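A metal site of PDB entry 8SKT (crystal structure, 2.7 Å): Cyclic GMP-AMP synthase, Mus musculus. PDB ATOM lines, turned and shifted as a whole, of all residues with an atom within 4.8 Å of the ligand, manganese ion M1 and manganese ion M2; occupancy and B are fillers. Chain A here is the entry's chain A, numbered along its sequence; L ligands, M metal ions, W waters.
An oxygen (O13) of the ligand is in hydrogen-bond range of the side-chain carboxylate (OE1) of Glu 228 (2.4 Å). O1 of the ligand is in hydrogen-bond range of OG of Ser 56. NZ of Lys 281 sits at hydrogen-bond distance from O12 of the ligand (3.1 Å). O3 of the ligand sits at hydrogen-bond distance from OG of Ser 277 (2.7 Å). The side-chain hydroxyl (OG) of Ser 225 is in hydrogen-bond range of an oxygen (O13) of the ligand (2.7 Å). An oxygen (O5) of the ligand lies close to the backbone NH (N) of Ser 56 (2.8 Å). NH2 of Arg 221 is in hydrogen-bond range of N5 of the ligand (3.0 Å). The side-chain amino group (NZ) of Lys 259 lies within salt-bridge range of an oxygen (O1) of the ligand.
OH of Tyr 278 sits at hydrogen-bond distance from OE2 of Glu 228 (2.6 Å). The side-chain carboxylate (OE1) of Glu 228 is in salt-bridge range of the side-chain amino group (NZ) of Lys 281, at 2.8 Å. OE2 of Glu 59 is in salt-bridge range of NZ of Lys 281 (2.7 Å). The side-chain sulfur (SG) of Cys 276 sits close to the backbone NH (N) of Tyr 278, at 3.7 Å. O of Ser 56 lies within hydrogen-bond range of N of Lys 62 (3.3 Å).
Gly 55 touches the ligand (CA to O5, 3.4 Å). Tyr 278 touches the ligand (CE2 to C9, 3.5 Å). Hydrophobic or aromatic side chains that line the ligand: Tyr 278. The nearest printed residue that does not touch the ligand is Lys 62 (4.1 Å).
Of the 17 residues printed, 3 come within 4 Å of manganese ion M1.
Residues that only touch manganese ion M2: Ser 56 (3.2 Å). Of the 17 residues printed, 3 come within 4 Å of manganese ion M2. The nearest printed residue that does not touch manganese ion M2 is Gly 55 (4.8 Å).
OE2 of Glu 68 is bound to manganese ion M1 (2.2 Å). OD1 of Asp 70 is bound to manganese ion M1 (2.2 Å). Manganese ion M1 is bound by OD2 of Asp 164. An oxygen (O8) of the ligand binds manganese ion M1, 2.5 Å away. Manganese ion M1 has four donor atoms within binding distance.
Manganese ion M2 is bound by the side-chain carboxylate (OE1) of Glu 68, the side-chain carboxylate (OD2) of Asp 70, an oxygen (O2) of the ligand, an oxygen (O5) of the ligand and an oxygen (O8) of the ligand.
Water W2 lies within hydrogen-bond range of O1 of the ligand (2.6 Å), OE2 of Glu 263 (3.2 Å) and NZ of Lys 62 (3.2 Å). Water W1 lies within hydrogen-bond range of O4 of the ligand, OG of Ser 277 and N of Tyr 278. Water W5 bridges OE1 of Glu 59 (2.5 Å) and O4 of the ligand (2.8 Å). Water W4 lies within hydrogen-bond range of O7 of the ligand (3.0 Å), OG of Ser 277 (3.0 Å), N of Tyr 278 (3.0 Å) and SG of Cys 276 (3.4 Å). Water W3 bridges the backbone NH (N) of Asp 70 and the backbone NH (N) of Ser 56.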
ATOM      1  N   GLY A  55      29.239  27.221  27.639  1.00  0.00           N
ATOM      2  CA  GLY A  55      28.321  28.308  27.764  1.00  0.00           C
ATOM      3  C   GLY A  55      28.753  29.529  26.997  1.00  0.00           C
ATOM      4  O   GLY A  55      29.716  29.524  26.228  1.00  0.00           O
ATOM      5  N   SER A  56      28.008  30.620  27.232  1.00  0.00           N
ATOM      6  CA  SER A  56      28.076  31.748  26.318  1.00  0.00           C
ATOM      7  C   SER A  56      29.477  32.326  26.264  1.00  0.00           C
ATOM      8  O   SER A  56      29.983  32.636  25.178  1.00  0.00           O
ATOM      9  CB  SER A  56      27.061  32.836  26.721  1.00  0.00           C
ATOM     10  OG  SER A  56      27.159  33.178  28.099  1.00  0.00           O
ATOM     11  N   GLU A  59      31.754  30.483  24.142  1.00  0.00           N
ATOM     12  CA  GLU A  59      31.316  30.408  22.764  1.00  0.00           C
ATOM     13  C   GLU A  59      31.459  31.746  22.053  1.00  0.00           C
ATOM     14  O   GLU A  59      31.259  31.810  20.836  1.00  0.00           O
ATOM     15  CB  GLU A  59      29.883  29.897  22.707  1.00  0.00           C
ATOM     16  CG  GLU A  59      29.703  28.452  23.152  1.00  0.00           C
ATOM     17  CD  GLU A  59      28.262  28.130  23.593  1.00  0.00           C
ATOM     18  OE1 GLU A  59      27.485  29.058  23.903  1.00  0.00           O
ATOM     19  OE2 GLU A  59      27.875  26.941  23.580  1.00  0.00           O
ATOM     20  N   LYS A  62      28.428  35.504  24.807  1.00  0.00           N
ATOM     21  CA  LYS A  62      28.092  36.256  26.012  1.00  0.00           C
ATOM     22  C   LYS A  62      27.961  37.747  25.711  1.00  0.00           C
ATOM     23  O   LYS A  62      28.844  38.330  25.087  1.00  0.00           O
ATOM     24  CB  LYS A  62      29.171  36.017  27.063  1.00  0.00           C
ATOM     25  CG  LYS A  62      29.055  36.901  28.272  1.00  0.00           C
ATOM     26  CD  LYS A  62      28.027  36.351  29.239  1.00  0.00           C
ATOM     27  CE  LYS A  62      27.162  37.482  29.699  1.00  0.00           C
ATOM     28  NZ  LYS A  62      26.366  37.178  30.904  1.00  0.00           N
ATOM     29  N   GLU A  68      28.721  36.266  33.745  1.00  0.00           N
ATOM     30  CA  GLU A  68      28.244  34.925  34.079  1.00  0.00           C
ATOM     31  C   GLU A  68      29.061  33.911  33.293  1.00  0.00           C
ATOM     32  O   GLU A  68      29.173  34.014  32.070  1.00  0.00           O
ATOM     33  CB  GLU A  68      26.754  34.770  33.795  1.00  0.00           C
ATOM     34  CG  GLU A  68      26.108  33.682  34.595  1.00  0.00           C
ATOM     35  CD  GLU A  68      26.009  32.380  33.809  1.00  0.00           C
ATOM     36  OE1 GLU A  68      26.608  32.326  32.719  1.00  0.00           O
ATOM     37  OE2 GLU A  68      25.331  31.423  34.283  1.00  0.00           O
ATOM     38  N   ASP A  70      30.069  29.635  32.897  1.00  0.00           N
ATOM     39  CA  ASP A  70      29.603  28.290  33.223  1.00  0.00           C
ATOM     40  C   ASP A  70      30.756  27.317  33.028  1.00  0.00           C
ATOM     41  O   ASP A  70      31.384  27.303  31.974  1.00  0.00           O
ATOM     42  CB  ASP A  70      28.415  27.870  32.381  1.00  0.00           C
ATOM     43  CG  ASP A  70      27.381  28.956  32.237  1.00  0.00           C
ATOM     44  OD1 ASP A  70      26.674  29.292  33.219  1.00  0.00           O
ATOM     45  OD2 ASP A  70      27.261  29.487  31.121  1.00  0.00           O
ATOM     46  N   ASP A 164      28.673  29.274  37.441  1.00  0.00           N
ATOM     47  CA  ASP A 164      27.974  28.035  37.683  1.00  0.00           C
ATOM     48  C   ASP A 164      28.980  26.900  37.621  1.00  0.00           C
ATOM     49  O   ASP A 164      29.481  26.569  36.543  1.00  0.00           O
ATOM     50  CB  ASP A 164      26.862  27.856  36.657  1.00  0.00           C
ATOM     51  CG  ASP A 164      25.656  28.701  36.976  1.00  0.00           C
ATOM     52  OD1 ASP A 164      25.381  28.920  38.178  1.00  0.00           O
ATOM     53  OD2 ASP A 164      24.992  29.145  36.020  1.00  0.00           O
ATOM     54  N   ARG A 221      20.003  14.274  34.078  1.00  0.00           N
ATOM     55  CA  ARG A 221      19.614  14.886  32.805  1.00  0.00           C
ATOM     56  C   ARG A 221      20.817  14.916  31.855  1.00  0.00           C
ATOM     57  O   ARG A 221      21.940  15.238  32.264  1.00  0.00           O
ATOM     58  CB  ARG A 221      19.087  16.315  33.023  1.00  0.00           C
ATOM     59  CG  ARG A 221      18.489  17.001  31.794  1.00  0.00           C
ATOM     60  CD  ARG A 221      18.580  18.531  31.883  1.00  0.00           C
ATOM     61  NE  ARG A 221      19.734  19.043  31.138  1.00  0.00           N
ATOM     62  CZ  ARG A 221      20.531  20.022  31.554  1.00  0.00           C
ATOM     63  NH1 ARG A 221      20.342  20.648  32.705  1.00  0.00           N
ATOM     64  NH2 ARG A 221      21.567  20.385  30.783  1.00  0.00           N
ATOM     65  N   SER A 225      26.462  20.426  26.373  1.00  0.00           N
ATOM     66  CA  SER A 225      27.164  21.696  26.339  1.00  0.00           C
ATOM     67  C   SER A 225      28.453  21.594  25.545  1.00  0.00           C
ATOM     68  O   SER A 225      28.861  22.560  24.893  1.00  0.00           O
ATOM     69  CB  SER A 225      27.486  22.159  27.752  1.00  0.00           C
ATOM     70  OG  SER A 225      26.379  22.782  28.348  1.00  0.00           O
ATOM     71  N   GLU A 228      27.570  21.640  21.851  1.00  0.00           N
ATOM     72  CA  GLU A 228      27.096  22.961  21.474  1.00  0.00           C
ATOM     73  C   GLU A 228      28.240  23.956  21.372  1.00  0.00           C
ATOM     74  O   GLU A 228      28.258  24.815  20.485  1.00  0.00           O
ATOM     75  CB  GLU A 228      26.050  23.420  22.478  1.00  0.00           C
ATOM     76  CG  GLU A 228      24.900  22.458  22.634  1.00  0.00           C
ATOM     77  CD  GLU A 228      24.092  22.766  23.849  1.00  0.00           C
ATOM     78  OE1 GLU A 228      24.441  23.743  24.545  1.00  0.00           O
ATOM     79  OE2 GLU A 228      23.078  22.079  24.104  1.00  0.00           O
ATOM     80  N   LYS A 259      19.204  36.680  22.113  1.00  0.00           N
ATOM     81  CA  LYS A 259      19.500  36.579  23.530  1.00  0.00           C
ATOM     82  C   LYS A 259      19.118  37.860  24.250  1.00  0.00           C
ATOM     83  O   LYS A 259      18.545  37.841  25.357  1.00  0.00           O
ATOM     84  CB  LYS A 259      20.989  36.312  23.735  1.00  0.00           C
ATOM     85  CG  LYS A 259      21.423  34.881  23.669  1.00  0.00           C
ATOM     86  CD  LYS A 259      22.946  34.846  23.561  1.00  0.00           C
ATOM     87  CE  LYS A 259      23.612  35.174  24.886  1.00  0.00           C
ATOM     88  NZ  LYS A 259      23.657  33.970  25.773  1.00  0.00           N
ATOM     89  N   GLU A 263      16.554  38.642  27.223  1.00  0.00           N
ATOM     90  CA  GLU A 263      17.090  39.177  28.483  1.00  0.00           C
ATOM     91  C   GLU A 263      16.385  40.475  28.887  1.00  0.00           C
ATOM     92  O   GLU A 263      15.921  40.602  30.024  1.00  0.00           O
ATOM     93  CB  GLU A 263      18.603  39.410  28.372  1.00  0.00           C
ATOM     94  CG  GLU A 263      19.455  38.187  28.645  1.00  0.00           C
ATOM     95  CD  GLU A 263      20.954  38.502  28.787  1.00  0.00           C
ATOM     96  OE1 GLU A 263      21.282  39.600  29.306  1.00  0.00           O
ATOM     97  OE2 GLU A 263      21.807  37.649  28.427  1.00  0.00           O
ATOM     98  N   CYS A 276      14.222  30.851  29.219  1.00  0.00           N
ATOM     99  CA  CYS A 276      15.639  31.025  29.480  1.00  0.00           C
ATOM    100  C   CYS A 276      16.340  31.116  28.138  1.00  0.00           C
ATOM    101  O   CYS A 276      15.745  30.871  27.084  1.00  0.00           O
ATOM    102  CB  CYS A 276      16.193  29.883  30.335  1.00  0.00           C
ATOM    103  SG  CYS A 276      16.159  28.301  29.496  1.00  0.00           S
ATOM    104  N   SER A 277      17.628  31.442  28.176  1.00  0.00           N
ATOM    105  CA  SER A 277      18.346  31.652  26.930  1.00  0.00           C
ATOM    106  C   SER A 277      18.566  30.349  26.174  1.00  0.00           C
ATOM    107  O   SER A 277      18.761  30.388  24.951  1.00  0.00           O
ATOM    108  CB  SER A 277      19.674  32.339  27.184  1.00  0.00           C
ATOM    109  OG  SER A 277      20.470  31.548  28.041  1.00  0.00           O
ATOM    110  N   TYR A 278      18.553  29.208  26.868  1.00  0.00           N
ATOM    111  CA  TYR A 278      18.711  27.951  26.155  1.00  0.00           C
ATOM    112  C   TYR A 278      17.585  27.754  25.167  1.00  0.00           C
ATOM    113  O   TYR A 278      17.744  27.030  24.173  1.00  0.00           O
ATOM    114  CB  TYR A 278      18.749  26.775  27.120  1.00  0.00           C
ATOM    115  CG  TYR A 278      19.172  25.477  26.430  1.00  0.00           C
ATOM    116  CD1 TYR A 278      20.467  25.338  25.934  1.00  0.00           C
ATOM    117  CD2 TYR A 278      18.284  24.414  26.272  1.00  0.00           C
ATOM    118  CE1 TYR A 278      20.876  24.180  25.306  1.00  0.00           C
ATOM    119  CE2 TYR A 278      18.688  23.228  25.630  1.00  0.00           C
ATOM    120  CZ  TYR A 278      20.000  23.124  25.159  1.00  0.00           C
ATOM    121  OH  TYR A 278      20.470  21.972  24.552  1.00  0.00           O
ATOM    122  N   LYS A 281      18.760  29.497  22.221  1.00  0.00           N
ATOM    123  CA  LYS A 281      19.888  28.747  21.662  1.00  0.00           C
ATOM    124  C   LYS A 281      19.381  27.577  20.840  1.00  0.00           C
ATOM    125  O   LYS A 281      19.858  27.325  19.721  1.00  0.00           O
ATOM    126  CB  LYS A 281      20.803  28.238  22.771  1.00  0.00           C
ATOM    127  CG  LYS A 281      22.196  27.868  22.314  1.00  0.00           C
ATOM    128  CD  LYS A 281      22.979  27.290  23.486  1.00  0.00           C
ATOM    129  CE  LYS A 281      24.479  27.472  23.307  1.00  0.00           C
ATOM    130  NZ  LYS A 281      25.261  26.385  24.001  1.00  0.00           N
ATOM    131  N   HIS A 324      14.062  19.698  21.727  1.00  0.00           N
ATOM    132  CA  HIS A 324      15.475  19.627  22.044  1.00  0.00           C
ATOM    133  C   HIS A 324      16.259  19.266  20.794  1.00  0.00           C
ATOM    134  O   HIS A 324      15.878  18.369  20.037  1.00  0.00           O
ATOM    135  CB  HIS A 324      15.691  18.576  23.144  1.00  0.00           C
ATOM    136  CG  HIS A 324      16.962  18.760  23.912  1.00  0.00           C
ATOM    137  ND1 HIS A 324      18.208  18.555  23.360  1.00  0.00           N
ATOM    138  CD2 HIS A 324      17.171  19.121  25.204  1.00  0.00           C
ATOM    139  CE1 HIS A 324      19.127  18.784  24.282  1.00  0.00           C
ATOM    140  NE2 HIS A 324      18.529  19.115  25.409  1.00  0.00           N
HETATM  141  P1  LIG L   1      23.881  33.061  28.960  1.00  0.00           P
HETATM  142  O1  LIG L   1      24.620  34.262  28.462  1.00  0.00           O
HETATM  143  O2  LIG L   1      24.377  32.592  30.316  1.00  0.00           O
HETATM  144  O3  LIG L   1      22.364  33.247  29.070  1.00  0.00           O
HETATM  145  P2  LIG L   1      24.363  30.267  28.165  1.00  0.00           P
HETATM  146  O4  LIG L   1      24.177  29.441  26.939  1.00  0.00           O
HETATM  147  O5  LIG L   1      25.720  30.161  28.832  1.00  0.00           O
HETATM  148  O6  LIG L   1      24.067  31.793  28.018  1.00  0.00           O
HETATM  149  P3  LIG L   1      23.336  29.272  30.692  1.00  0.00           P
HETATM  150  O7  LIG L   1      21.983  29.237  31.272  1.00  0.00           O
HETATM  151  O8  LIG L   1      24.469  30.039  31.367  1.00  0.00           O
HETATM  152  O9  LIG L   1      23.292  29.852  29.263  1.00  0.00           O
HETATM  153  O10 LIG L   1      23.615  27.723  30.468  1.00  0.00           O
HETATM  154  C1  LIG L   1      24.937  27.206  30.256  1.00  0.00           C
HETATM  155  C2  LIG L   1      24.821  26.022  29.329  1.00  0.00           C
HETATM  156  O11 LIG L   1      24.146  24.905  29.979  1.00  0.00           O
HETATM  157  C3  LIG L   1      24.005  26.272  28.066  1.00  0.00           C
HETATM  158  O12 LIG L   1      24.827  26.840  27.051  1.00  0.00           O
HETATM  159  C4  LIG L   1      23.554  24.859  27.671  1.00  0.00           C
HETATM  160  O13 LIG L   1      24.554  24.195  26.910  1.00  0.00           O
HETATM  161  C5  LIG L   1      23.324  24.213  29.051  1.00  0.00           C
HETATM  162  N1  LIG L   1      21.940  24.343  29.475  1.00  0.00           N
HETATM  163  C6  LIG L   1      21.378  25.404  30.134  1.00  0.00           C
HETATM  164  N2  LIG L   1      20.094  25.286  30.355  1.00  0.00           N
HETATM  165  C7  LIG L   1      19.777  24.064  29.787  1.00  0.00           C
HETATM  166  C8  LIG L   1      18.571  23.346  29.680  1.00  0.00           C
HETATM  167  N3  LIG L   1      17.404  23.775  30.169  1.00  0.00           N
HETATM  168  N4  LIG L   1      18.597  22.147  29.048  1.00  0.00           N
HETATM  169  C9  LIG L   1      19.765  21.710  28.552  1.00  0.00           C
HETATM  170  N5  LIG L   1      20.961  22.307  28.584  1.00  0.00           N
HETATM  171  C10 LIG L   1      20.906  23.478  29.230  1.00  0.00           C
HETATM  172 MN    MN M   1      24.515  29.424  33.804  1.00  0.00          MN
HETATM  173 MN    MN M   2      26.330  31.494  30.704  1.00  0.00          MN
HETATM  174  O   HOH W   1      21.568  29.334  26.341  1.00  0.00           O
HETATM  175  O   HOH W   2      24.863  36.817  28.085  1.00  0.00           O
HETATM  176  O   HOH W   3      29.681  30.626  30.249  1.00  0.00           O
HETATM  177  O   HOH W   4      19.443  29.329  29.733  1.00  0.00           O
HETATM  178  O   HOH W   5      25.321  30.238  24.544  1.00  0.00           O
